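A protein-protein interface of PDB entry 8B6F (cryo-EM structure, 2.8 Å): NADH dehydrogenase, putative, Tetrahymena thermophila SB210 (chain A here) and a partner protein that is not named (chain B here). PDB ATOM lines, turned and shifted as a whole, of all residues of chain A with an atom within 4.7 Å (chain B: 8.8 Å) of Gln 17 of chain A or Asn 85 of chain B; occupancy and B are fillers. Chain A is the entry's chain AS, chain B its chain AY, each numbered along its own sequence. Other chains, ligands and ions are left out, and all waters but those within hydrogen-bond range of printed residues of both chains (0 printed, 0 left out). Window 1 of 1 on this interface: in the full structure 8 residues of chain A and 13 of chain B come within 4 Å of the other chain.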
ATOM      1  N   PRO A  12     -21.377 -18.081 -12.007  1.00  0.00           N
ATOM      2  CA  PRO A  12     -21.692 -18.700 -13.301  1.00  0.00           C
ATOM      3  C   PRO A  12     -20.850 -19.942 -13.546  1.00  0.00           C
ATOM      4  O   PRO A  12     -19.672 -19.998 -13.189  1.00  0.00           O
ATOM      5  CB  PRO A  12     -21.368 -17.595 -14.312  1.00  0.00           C
ATOM      6  CG  PRO A  12     -21.449 -16.335 -13.543  1.00  0.00           C
ATOM      7  CD  PRO A  12     -20.988 -16.669 -12.159  1.00  0.00           C
ATOM      8  N   ALA A  13     -21.470 -20.947 -14.165  1.00  0.00           N
ATOM      9  CA  ALA A  13     -20.761 -22.182 -14.470  1.00  0.00           C
ATOM     10  C   ALA A  13     -19.845 -22.053 -15.676  1.00  0.00           C
ATOM     11  O   ALA A  13     -18.972 -22.905 -15.867  1.00  0.00           O
ATOM     12  CB  ALA A  13     -21.759 -23.315 -14.711  1.00  0.00           C
ATOM     13  N   SER A  14     -20.023 -21.017 -16.491  1.00  0.00           N
ATOM     14  CA  SER A  14     -19.218 -20.844 -17.687  1.00  0.00           C
ATOM     15  C   SER A  14     -19.039 -19.358 -17.948  1.00  0.00           C
ATOM     16  O   SER A  14     -19.770 -18.521 -17.413  1.00  0.00           O
ATOM     17  CB  SER A  14     -19.865 -21.529 -18.898  1.00  0.00           C
ATOM     18  OG  SER A  14     -19.084 -21.356 -20.066  1.00  0.00           O
ATOM     19  N   SER A  15     -18.047 -19.039 -18.778  1.00  0.00           N
ATOM     20  CA  SER A  15     -17.798 -17.646 -19.133  1.00  0.00           C
ATOM     21  C   SER A  15     -18.950 -17.049 -19.924  1.00  0.00           C
ATOM     22  O   SER A  15     -19.180 -15.836 -19.860  1.00  0.00           O
ATOM     23  CB  SER A  15     -16.499 -17.528 -19.917  1.00  0.00           C
ATOM     24  OG  SER A  15     -15.434 -18.051 -19.152  1.00  0.00           O
ATOM     25  N   THR A  16     -19.678 -17.876 -20.676  1.00  0.00           N
ATOM     26  CA  THR A  16     -20.738 -17.402 -21.555  1.00  0.00           C
ATOM     27  C   THR A  16     -22.092 -18.023 -21.237  1.00  0.00           C
ATOM     28  O   THR A  16     -23.032 -17.858 -22.021  1.00  0.00           O
ATOM     29  CB  THR A  16     -20.377 -17.691 -23.017  1.00  0.00           C
ATOM     30  OG1 THR A  16     -20.179 -19.100 -23.195  1.00  0.00           O
ATOM     31  CG2 THR A  16     -19.107 -16.956 -23.415  1.00  0.00           C
ATOM     32  N   GLN A  17     -22.226 -18.722 -20.113  1.00  0.00           N
ATOM     33  CA  GLN A  17     -23.467 -19.419 -19.804  1.00  0.00           C
ATOM     34  C   GLN A  17     -23.587 -19.590 -18.299  1.00  0.00           C
ATOM     35  O   GLN A  17     -22.624 -19.414 -17.552  1.00  0.00           O
ATOM     36  CB  GLN A  17     -23.531 -20.786 -20.491  1.00  0.00           C
ATOM     37  CG  GLN A  17     -23.953 -20.737 -21.938  1.00  0.00           C
ATOM     38  CD  GLN A  17     -24.146 -22.117 -22.518  1.00  0.00           C
ATOM     39  OE1 GLN A  17     -23.613 -23.096 -22.003  1.00  0.00           O
ATOM     40  NE2 GLN A  17     -24.925 -22.204 -23.587  1.00  0.00           N
ATOM     41  N   ASN A  18     -24.798 -19.936 -17.866  1.00  0.00           N
ATOM     42  CA  ASN A  18     -25.070 -20.372 -16.498  1.00  0.00           C
ATOM     43  C   ASN A  18     -25.534 -21.826 -16.568  1.00  0.00           C
ATOM     44  O   ASN A  18     -26.732 -22.117 -16.589  1.00  0.00           O
ATOM     45  CB  ASN A  18     -26.115 -19.475 -15.825  1.00  0.00           C
ATOM     46  CG  ASN A  18     -25.651 -18.041 -15.687  1.00  0.00           C
ATOM     47  OD1 ASN A  18     -24.457 -17.757 -15.738  1.00  0.00           O
ATOM     48  ND2 ASN A  18     -26.596 -17.128 -15.502  1.00  0.00           N
ATOM     49  N   ASN A  19     -24.568 -22.738 -16.613  1.00  0.00           N
ATOM     50  CA  ASN A  19     -24.796 -24.159 -16.376  1.00  0.00           C
ATOM     51  C   ASN A  19     -25.505 -24.885 -17.516  1.00  0.00           C
ATOM     52  O   ASN A  19     -25.626 -26.113 -17.468  1.00  0.00           O
ATOM     53  CB  ASN A  19     -25.599 -24.352 -15.086  1.00  0.00           C
ATOM     54  CG  ASN A  19     -27.032 -24.758 -15.351  1.00  0.00           C
ATOM     55  OD1 ASN A  19     -27.356 -25.942 -15.389  1.00  0.00           O
ATOM     56  ND2 ASN A  19     -27.900 -23.774 -15.537  1.00  0.00           N
ATOM     57  N   ASN A  20     -25.961 -24.175 -18.545  1.00  0.00           N
ATOM     58  CA  ASN A  20     -26.700 -24.831 -19.621  1.00  0.00           C
ATOM     59  C   ASN A  20     -27.003 -23.820 -20.718  1.00  0.00           C
ATOM     60  O   ASN A  20     -26.841 -22.611 -20.539  1.00  0.00           O
ATOM     61  CB  ASN A  20     -28.010 -25.451 -19.126  1.00  0.00           C
ATOM     62  CG  ASN A  20     -27.890 -26.932 -18.858  1.00  0.00           C
ATOM     63  OD1 ASN A  20     -27.115 -27.631 -19.505  1.00  0.00           O
ATOM     64  ND2 ASN A  20     -28.661 -27.422 -17.894  1.00  0.00           N
ATOM     65  N   TYR A  21     -27.460 -24.341 -21.855  1.00  0.00           N
ATOM     66  CA  TYR A  21     -27.922 -23.524 -22.968  1.00  0.00           C
ATOM     67  C   TYR A  21     -29.434 -23.351 -22.983  1.00  0.00           C
ATOM     68  O   TYR A  21     -29.934 -22.478 -23.697  1.00  0.00           O
ATOM     69  CB  TYR A  21     -27.472 -24.136 -24.301  1.00  0.00           C
ATOM     70  CG  TYR A  21     -28.253 -25.361 -24.723  1.00  0.00           C
ATOM     71  CD1 TYR A  21     -27.906 -26.625 -24.265  1.00  0.00           C
ATOM     72  CD2 TYR A  21     -29.324 -25.254 -25.599  1.00  0.00           C
ATOM     73  CE1 TYR A  21     -28.614 -27.744 -24.654  1.00  0.00           C
ATOM     74  CE2 TYR A  21     -30.037 -26.366 -25.994  1.00  0.00           C
ATOM     75  CZ  TYR A  21     -29.676 -27.608 -25.520  1.00  0.00           C
ATOM     76  OH  TYR A  21     -30.385 -28.717 -25.913  1.00  0.00           O
ATOM     77  N   ALA B  78     -17.291 -14.122 -30.709  1.00  0.00           N
ATOM     78  CA  ALA B  78     -16.971 -14.880 -29.503  1.00  0.00           C
ATOM     79  C   ALA B  78     -17.435 -14.150 -28.249  1.00  0.00           C
ATOM     80  O   ALA B  78     -17.873 -14.781 -27.281  1.00  0.00           O
ATOM     81  CB  ALA B  78     -15.468 -15.148 -29.438  1.00  0.00           C
ATOM     82  N   ILE B  79     -17.329 -12.822 -28.240  1.00  0.00           N
ATOM     83  CA  ILE B  79     -17.822 -12.047 -27.106  1.00  0.00           C
ATOM     84  C   ILE B  79     -19.343 -12.060 -27.081  1.00  0.00           C
ATOM     85  O   ILE B  79     -19.962 -12.147 -26.015  1.00  0.00           O
ATOM     86  CB  ILE B  79     -17.254 -10.618 -27.147  1.00  0.00           C
ATOM     87  CG1 ILE B  79     -15.755 -10.662 -26.841  1.00  0.00           C
ATOM     88  CG2 ILE B  79     -17.990  -9.711 -26.159  1.00  0.00           C
ATOM     89  CD1 ILE B  79     -15.052  -9.344 -26.998  1.00  0.00           C
ATOM     90  N   LEU B  80     -19.967 -11.971 -28.253  1.00  0.00           N
ATOM     91  CA  LEU B  80     -21.418 -12.008 -28.334  1.00  0.00           C
ATOM     92  C   LEU B  80     -21.989 -13.335 -27.844  1.00  0.00           C
ATOM     93  O   LEU B  80     -23.161 -13.386 -27.462  1.00  0.00           O
ATOM     94  CB  LEU B  80     -21.845 -11.728 -29.774  1.00  0.00           C
ATOM     95  CG  LEU B  80     -23.336 -11.845 -30.058  1.00  0.00           C
ATOM     96  CD1 LEU B  80     -24.137 -10.769 -29.328  1.00  0.00           C
ATOM     97  CD2 LEU B  80     -23.615 -11.802 -31.549  1.00  0.00           C
ATOM     98  N   TYR B  81     -21.193 -14.404 -27.860  1.00  0.00           N
ATOM     99  CA  TYR B  81     -21.643 -15.684 -27.320  1.00  0.00           C
ATOM    100  C   TYR B  81     -22.204 -15.532 -25.910  1.00  0.00           C
ATOM    101  O   TYR B  81     -23.214 -16.154 -25.563  1.00  0.00           O
ATOM    102  CB  TYR B  81     -20.488 -16.689 -27.322  1.00  0.00           C
ATOM    103  CG  TYR B  81     -20.495 -17.650 -28.488  1.00  0.00           C
ATOM    104  CD1 TYR B  81     -19.942 -17.296 -29.711  1.00  0.00           C
ATOM    105  CD2 TYR B  81     -21.032 -18.921 -28.356  1.00  0.00           C
ATOM    106  CE1 TYR B  81     -19.941 -18.176 -30.774  1.00  0.00           C
ATOM    107  CE2 TYR B  81     -21.034 -19.810 -29.411  1.00  0.00           C
ATOM    108  CZ  TYR B  81     -20.486 -19.432 -30.617  1.00  0.00           C
ATOM    109  OH  TYR B  81     -20.489 -20.315 -31.669  1.00  0.00           O
ATOM    110  N   LYS B  82     -21.559 -14.710 -25.080  1.00  0.00           N
ATOM    111  CA  LYS B  82     -22.005 -14.538 -23.700  1.00  0.00           C
ATOM    112  C   LYS B  82     -23.422 -13.981 -23.634  1.00  0.00           C
ATOM    113  O   LYS B  82     -24.289 -14.546 -22.958  1.00  0.00           O
ATOM    114  CB  LYS B  82     -21.040 -13.621 -22.945  1.00  0.00           C
ATOM    115  CG  LYS B  82     -21.446 -13.365 -21.497  1.00  0.00           C
ATOM    116  CD  LYS B  82     -20.472 -12.442 -20.783  1.00  0.00           C
ATOM    117  CE  LYS B  82     -20.542 -11.026 -21.324  1.00  0.00           C
ATOM    118  NZ  LYS B  82     -19.677 -10.096 -20.545  1.00  0.00           N
ATOM    119  N   ASN B  83     -23.681 -12.870 -24.324  1.00  0.00           N
ATOM    120  CA  ASN B  83     -25.010 -12.273 -24.261  1.00  0.00           C
ATOM    121  C   ASN B  83     -26.071 -13.182 -24.864  1.00  0.00           C
ATOM    122  O   ASN B  83     -27.241 -13.107 -24.476  1.00  0.00           O
ATOM    123  CB  ASN B  83     -25.008 -10.920 -24.971  1.00  0.00           C
ATOM    124  CG  ASN B  83     -24.695  -9.773 -24.036  1.00  0.00           C
ATOM    125  OD1 ASN B  83     -24.131  -9.971 -22.963  1.00  0.00           O
ATOM    126  ND2 ASN B  83     -25.060  -8.564 -24.440  1.00  0.00           N
ATOM    127  N   LEU B  84     -25.696 -14.036 -25.807  1.00  0.00           N
ATOM    128  CA  LEU B  84     -26.634 -14.971 -26.412  1.00  0.00           C
ATOM    129  C   LEU B  84     -26.737 -16.288 -25.652  1.00  0.00           C
ATOM    130  O   LEU B  84     -27.546 -17.141 -26.028  1.00  0.00           O
ATOM    131  CB  LEU B  84     -26.246 -15.209 -27.873  1.00  0.00           C
ATOM    132  CG  LEU B  84     -26.994 -14.227 -28.778  1.00  0.00           C
ATOM    133  CD1 LEU B  84     -26.189 -13.816 -29.961  1.00  0.00           C
ATOM    134  CD2 LEU B  84     -28.280 -14.866 -29.248  1.00  0.00           C
ATOM    135  N   ASN B  85     -25.952 -16.467 -24.590  1.00  0.00           N
ATOM    136  CA  ASN B  85     -26.042 -17.653 -23.739  1.00  0.00           C
ATOM    137  C   ASN B  85     -25.755 -18.924 -24.534  1.00  0.00           C
ATOM    138  O   ASN B  85     -26.545 -19.870 -24.547  1.00  0.00           O
ATOM    139  CB  ASN B  85     -27.406 -17.727 -23.053  1.00  0.00           C
ATOM    140  CG  ASN B  85     -27.489 -18.861 -22.053  1.00  0.00           C
ATOM    141  OD1 ASN B  85     -27.982 -19.942 -22.362  1.00  0.00           O
ATOM    142  ND2 ASN B  85     -26.999 -18.617 -20.844  1.00  0.00           N
ATOM    143  N   GLU B  86     -24.609 -18.940 -25.205  1.00  0.00           N
ATOM    144  CA  GLU B  86     -24.164 -20.093 -25.971  1.00  0.00           C
ATOM    145  C   GLU B  86     -22.776 -20.494 -25.501  1.00  0.00           C
ATOM    146  O   GLU B  86     -21.898 -19.640 -25.347  1.00  0.00           O
ATOM    147  CB  GLU B  86     -24.145 -19.785 -27.470  1.00  0.00           C
ATOM    148  CG  GLU B  86     -25.515 -19.812 -28.125  1.00  0.00           C
ATOM    149  CD  GLU B  86     -26.075 -21.213 -28.256  1.00  0.00           C
ATOM    150  OE1 GLU B  86     -26.423 -21.821 -27.224  1.00  0.00           O
ATOM    151  OE2 GLU B  86     -26.158 -21.713 -29.398  1.00  0.00           O
ATOM    152  N   SER B  87     -22.587 -21.787 -25.263  1.00  0.00           N
ATOM    153  CA  SER B  87     -21.269 -22.289 -24.914  1.00  0.00           C
ATOM    154  C   SER B  87     -20.338 -22.178 -26.112  1.00  0.00           C
ATOM    155  O   SER B  87     -20.733 -22.438 -27.251  1.00  0.00           O
ATOM    156  CB  SER B  87     -21.362 -23.742 -24.454  1.00  0.00           C
ATOM    157  OG  SER B  87     -20.102 -24.228 -24.026  1.00  0.00           O
ATOM    158  N   LEU B  88     -19.093 -21.776 -25.853  1.00  0.00           N
ATOM    159  CA  LEU B  88     -18.109 -21.728 -26.926  1.00  0.00           C
ATOM    160  C   LEU B  88     -17.925 -23.097 -27.561  1.00  0.00           C
ATOM    161  O   LEU B  88     -17.701 -23.195 -28.773  1.00  0.00           O
ATOM    162  CB  LEU B  88     -16.778 -21.196 -26.397  1.00  0.00           C
ATOM    163  CG  LEU B  88     -16.769 -19.719 -25.993  1.00  0.00           C
ATOM    164  CD1 LEU B  88     -15.459 -19.362 -25.315  1.00  0.00           C
ATOM    165  CD2 LEU B  88     -17.002 -18.818 -27.194  1.00  0.00           C
ATOM    166  N   ASN B  89     -18.016 -24.159 -26.766  1.00  0.00           N
ATOM    167  CA  ASN B  89     -18.019 -25.521 -27.291  1.00  0.00           C
ATOM    168  C   ASN B  89     -19.389 -25.768 -27.907  1.00  0.00           C
ATOM    169  O   ASN B  89     -20.347 -26.098 -27.209  1.00  0.00           O
ATOM    170  CB  ASN B  89     -17.711 -26.525 -26.188  1.00  0.00           C
ATOM    171  CG  ASN B  89     -16.426 -26.205 -25.455  1.00  0.00           C
ATOM    172  OD1 ASN B  89     -15.333 -26.447 -25.961  1.00  0.00           O
ATOM    173  ND2 ASN B  89     -16.553 -25.666 -24.249  1.00  0.00           N
ATOM    174  N   THR B  90     -19.481 -25.609 -29.228  1.00  0.00           N
ATOM    175  CA  THR B  90     -20.781 -25.662 -29.886  1.00  0.00           C
ATOM    176  C   THR B  90     -21.469 -27.001 -29.674  1.00  0.00           C
ATOM    177  O   THR B  90     -22.703 -27.071 -29.665  1.00  0.00           O
ATOM    178  CB  THR B  90     -20.626 -25.383 -31.380  1.00  0.00           C
ATOM    179  OG1 THR B  90     -19.817 -26.401 -31.980  1.00  0.00           O
ATOM    180  CG2 THR B  90     -19.981 -24.023 -31.609  1.00  0.00           C
ATOM    181  N   LEU B  92     -22.006 -28.567 -27.128  1.00  0.00           N
ATOM    182  CA  LEU B  92     -22.830 -28.543 -25.927  1.00  0.00           C
ATOM    183  C   LEU B  92     -24.092 -27.708 -26.089  1.00  0.00           C
ATOM    184  O   LEU B  92     -24.865 -27.593 -25.134  1.00  0.00           O
ATOM    185  CB  LEU B  92     -22.019 -28.010 -24.740  1.00  0.00           C
ATOM    186  CG  LEU B  92     -20.847 -28.865 -24.254  1.00  0.00           C
ATOM    187  CD1 LEU B  92     -20.123 -28.159 -23.122  1.00  0.00           C
ATOM    188  CD2 LEU B  92     -21.310 -30.243 -23.809  1.00  0.00           C
ATOM    189  N   ASN B  93     -24.318 -27.123 -27.262  1.00  0.00           N
ATOM    190  CA  ASN B  93     -25.500 -26.312 -27.512  1.00  0.00           C
ATOM    191  C   ASN B  93     -26.674 -27.126 -28.036  1.00  0.00           C
ATOM    192  O   ASN B  93     -27.718 -26.548 -28.351  1.00  0.00           O
ATOM    193  CB  ASN B  93     -25.172 -25.195 -28.507  1.00  0.00           C
ATOM    194  CG  ASN B  93     -24.148 -24.219 -27.969  1.00  0.00           C
ATOM    195  OD1 ASN B  93     -24.031 -24.028 -26.760  1.00  0.00           O
ATOM    196  ND2 ASN B  93     -23.398 -23.591 -28.867  1.00  0.00           N
ATOM    197  N   ASN B  94     -26.527 -28.444 -28.143  1.00  0.00           N
ATOM    198  CA  ASN B  94     -27.599 -29.318 -28.588  1.00  0.00           C
ATOM    199  C   ASN B  94     -27.603 -30.570 -27.726  1.00  0.00           C
ATOM    200  O   ASN B  94     -26.600 -30.923 -27.102  1.00  0.00           O
ATOM    201  CB  ASN B  94     -27.451 -29.687 -30.069  1.00  0.00           C
ATOM    202  CG  ASN B  94     -26.067 -30.198 -30.405  1.00  0.00           C
ATOM    203  OD1 ASN B  94     -25.732 -31.345 -30.123  1.00  0.00           O
ATOM    204  ND2 ASN B  94     -25.256 -29.346 -31.017  1.00  0.00           N
ATOM    205  N   PHE B 106     -27.778 -33.972 -20.351  1.00  0.00           N
ATOM    206  CA  PHE B 106     -28.758 -32.921 -20.113  1.00  0.00           C
ATOM    207  C   PHE B 106     -30.078 -33.536 -19.680  1.00  0.00           C
ATOM    208  O   PHE B 106     -30.492 -34.576 -20.201  1.00  0.00           O
ATOM    209  CB  PHE B 106     -28.977 -32.062 -21.366  1.00  0.00           C
ATOM    210  CG  PHE B 106     -27.791 -31.222 -21.748  1.00  0.00           C
ATOM    211  CD1 PHE B 106     -27.008 -30.612 -20.781  1.00  0.00           C
ATOM    212  CD2 PHE B 106     -27.464 -31.039 -23.079  1.00  0.00           C
ATOM    213  CE1 PHE B 106     -25.922 -29.840 -21.137  1.00  0.00           C
ATOM    214  CE2 PHE B 106     -26.379 -30.267 -23.440  1.00  0.00           C
ATOM    215  CZ  PHE B 106     -25.607 -29.668 -22.467  1.00  0.00           C
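O of Asn 20 of chain A sits close to OD1 of Asn 85 of chain B. The side-chain amide nitrogen of Gln 17 of chain A sits at hydrogen-bond distance from the backbone carbonyl oxygen of Asn 85 of chain B, at 3.0 Å. O of Tyr 21 of chain A lies close to OD1 of Asn 85 of chain B (3.5 Å). The side-chain hydroxyl (OG1) of Thr 16 of chain A lies within hydrogen-bond range of the backbone carbonyl oxygen (O) of Glu 86 of chain B (2.8 Å). The backbone NH of Ser 87 of chain B lies close to the side-chain amide nitrogen of Gln 17 of chain A (2.9 Å).
O of Tyr 81 of chain B lies within hydrogen-bond range of N of Glu 86 of chain B, 3.1 Å away. OG of Ser 87 of chain B sits close to N of Asn 89 of chain B (3.4 Å). The side-chain carboxylate (OE1) of Glu 86 of chain B lies close to the side-chain amide oxygen (OD1) of Asn 93 of chain B, 3.3 Å away. OD1 of Asn 93 of chain B lies within hydrogen-bond range of N of Ser 87 of chain B. The side-chain amide oxygen of Asn 19 of chain A lies within hydrogen-bond range of the side-chain amide nitrogen of Asn 20 of chain A, at 3.2 Å.
Among the printed residues, pairs that only touch across the chains: Ser 15 of chain A with Lys 82 of chain B, Thr 16 of chain A with Tyr 81 of chain B, Thr 16 of chain A with Lys 82 of chain B, Thr 16 of chain A with Asn 85 of chain B, Thr 16 of chain A with Ser 87 of chain B, Thr 16 of chain A with Leu 88 of chain B, Gln 17 of chain A with Glu 86 of chain B, Gln 17 of chain A with Asn 93 of chain B, Asn 18 of chain A with Asn 85 of chain B, Asn 20 of chain A with Phe 106 of chain B, Tyr 21 of chain A with Glu 86 of chain B, Tyr 21 of chain A with Leu 92 of chain B, Tyr 21 of chain A with Asn 93 of chain B, Tyr 21 of chain A with Asn 94 of chain B and Tyr 21 of chain A with Phe 106 of chain B.
Gln 17 of chain A touches just these residues of chain B: Asn 85, Glu 86, Ser 87 and Asn 93. Asn 85 of chain B touches five residues of chain A. No residue of chain B comes within 4 Å of Ser 14 of chain A. Of the printed residues of chain B, Tyr 21 of chain A touches Asn 85 (3.5 Å), Glu 86 (3.9 Å), Leu 92 (3.3 Å), Asn 93 (3.3 Å), Asn 94 (3.8 Å) and Phe 106 (3.6 Å). Of the printed residues of chain A, Tyr 81 of chain B touches Thr 16 (3.9 Å). Pro 12 of chain A touches none of the printed residues of chain B. The nearest residue of chain B that does not touch Gln 17 of chain A is Lys 82 of chain B (5.5 Å). The nearest printed residue of chain A that does not touch Glu 86 of chain B is Ser 14 of chain A (6.2 Å).
Of the 17 printed residues of chain B, 10 touch a printed residue of chain A. Of the 10 printed residues of chain A, 6 touch a printed residue of chain B. Hydrophobic or aromatic side chains of chain A within 4 Å of the printed part of chain B: Tyr 21. Among the printed residues, 20 pairs touch across the chains. Among the printed residues, no Asp or Glu carboxylate lies within 4 Å of a Lys or Arg side-chain nitrogen of the other chain.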
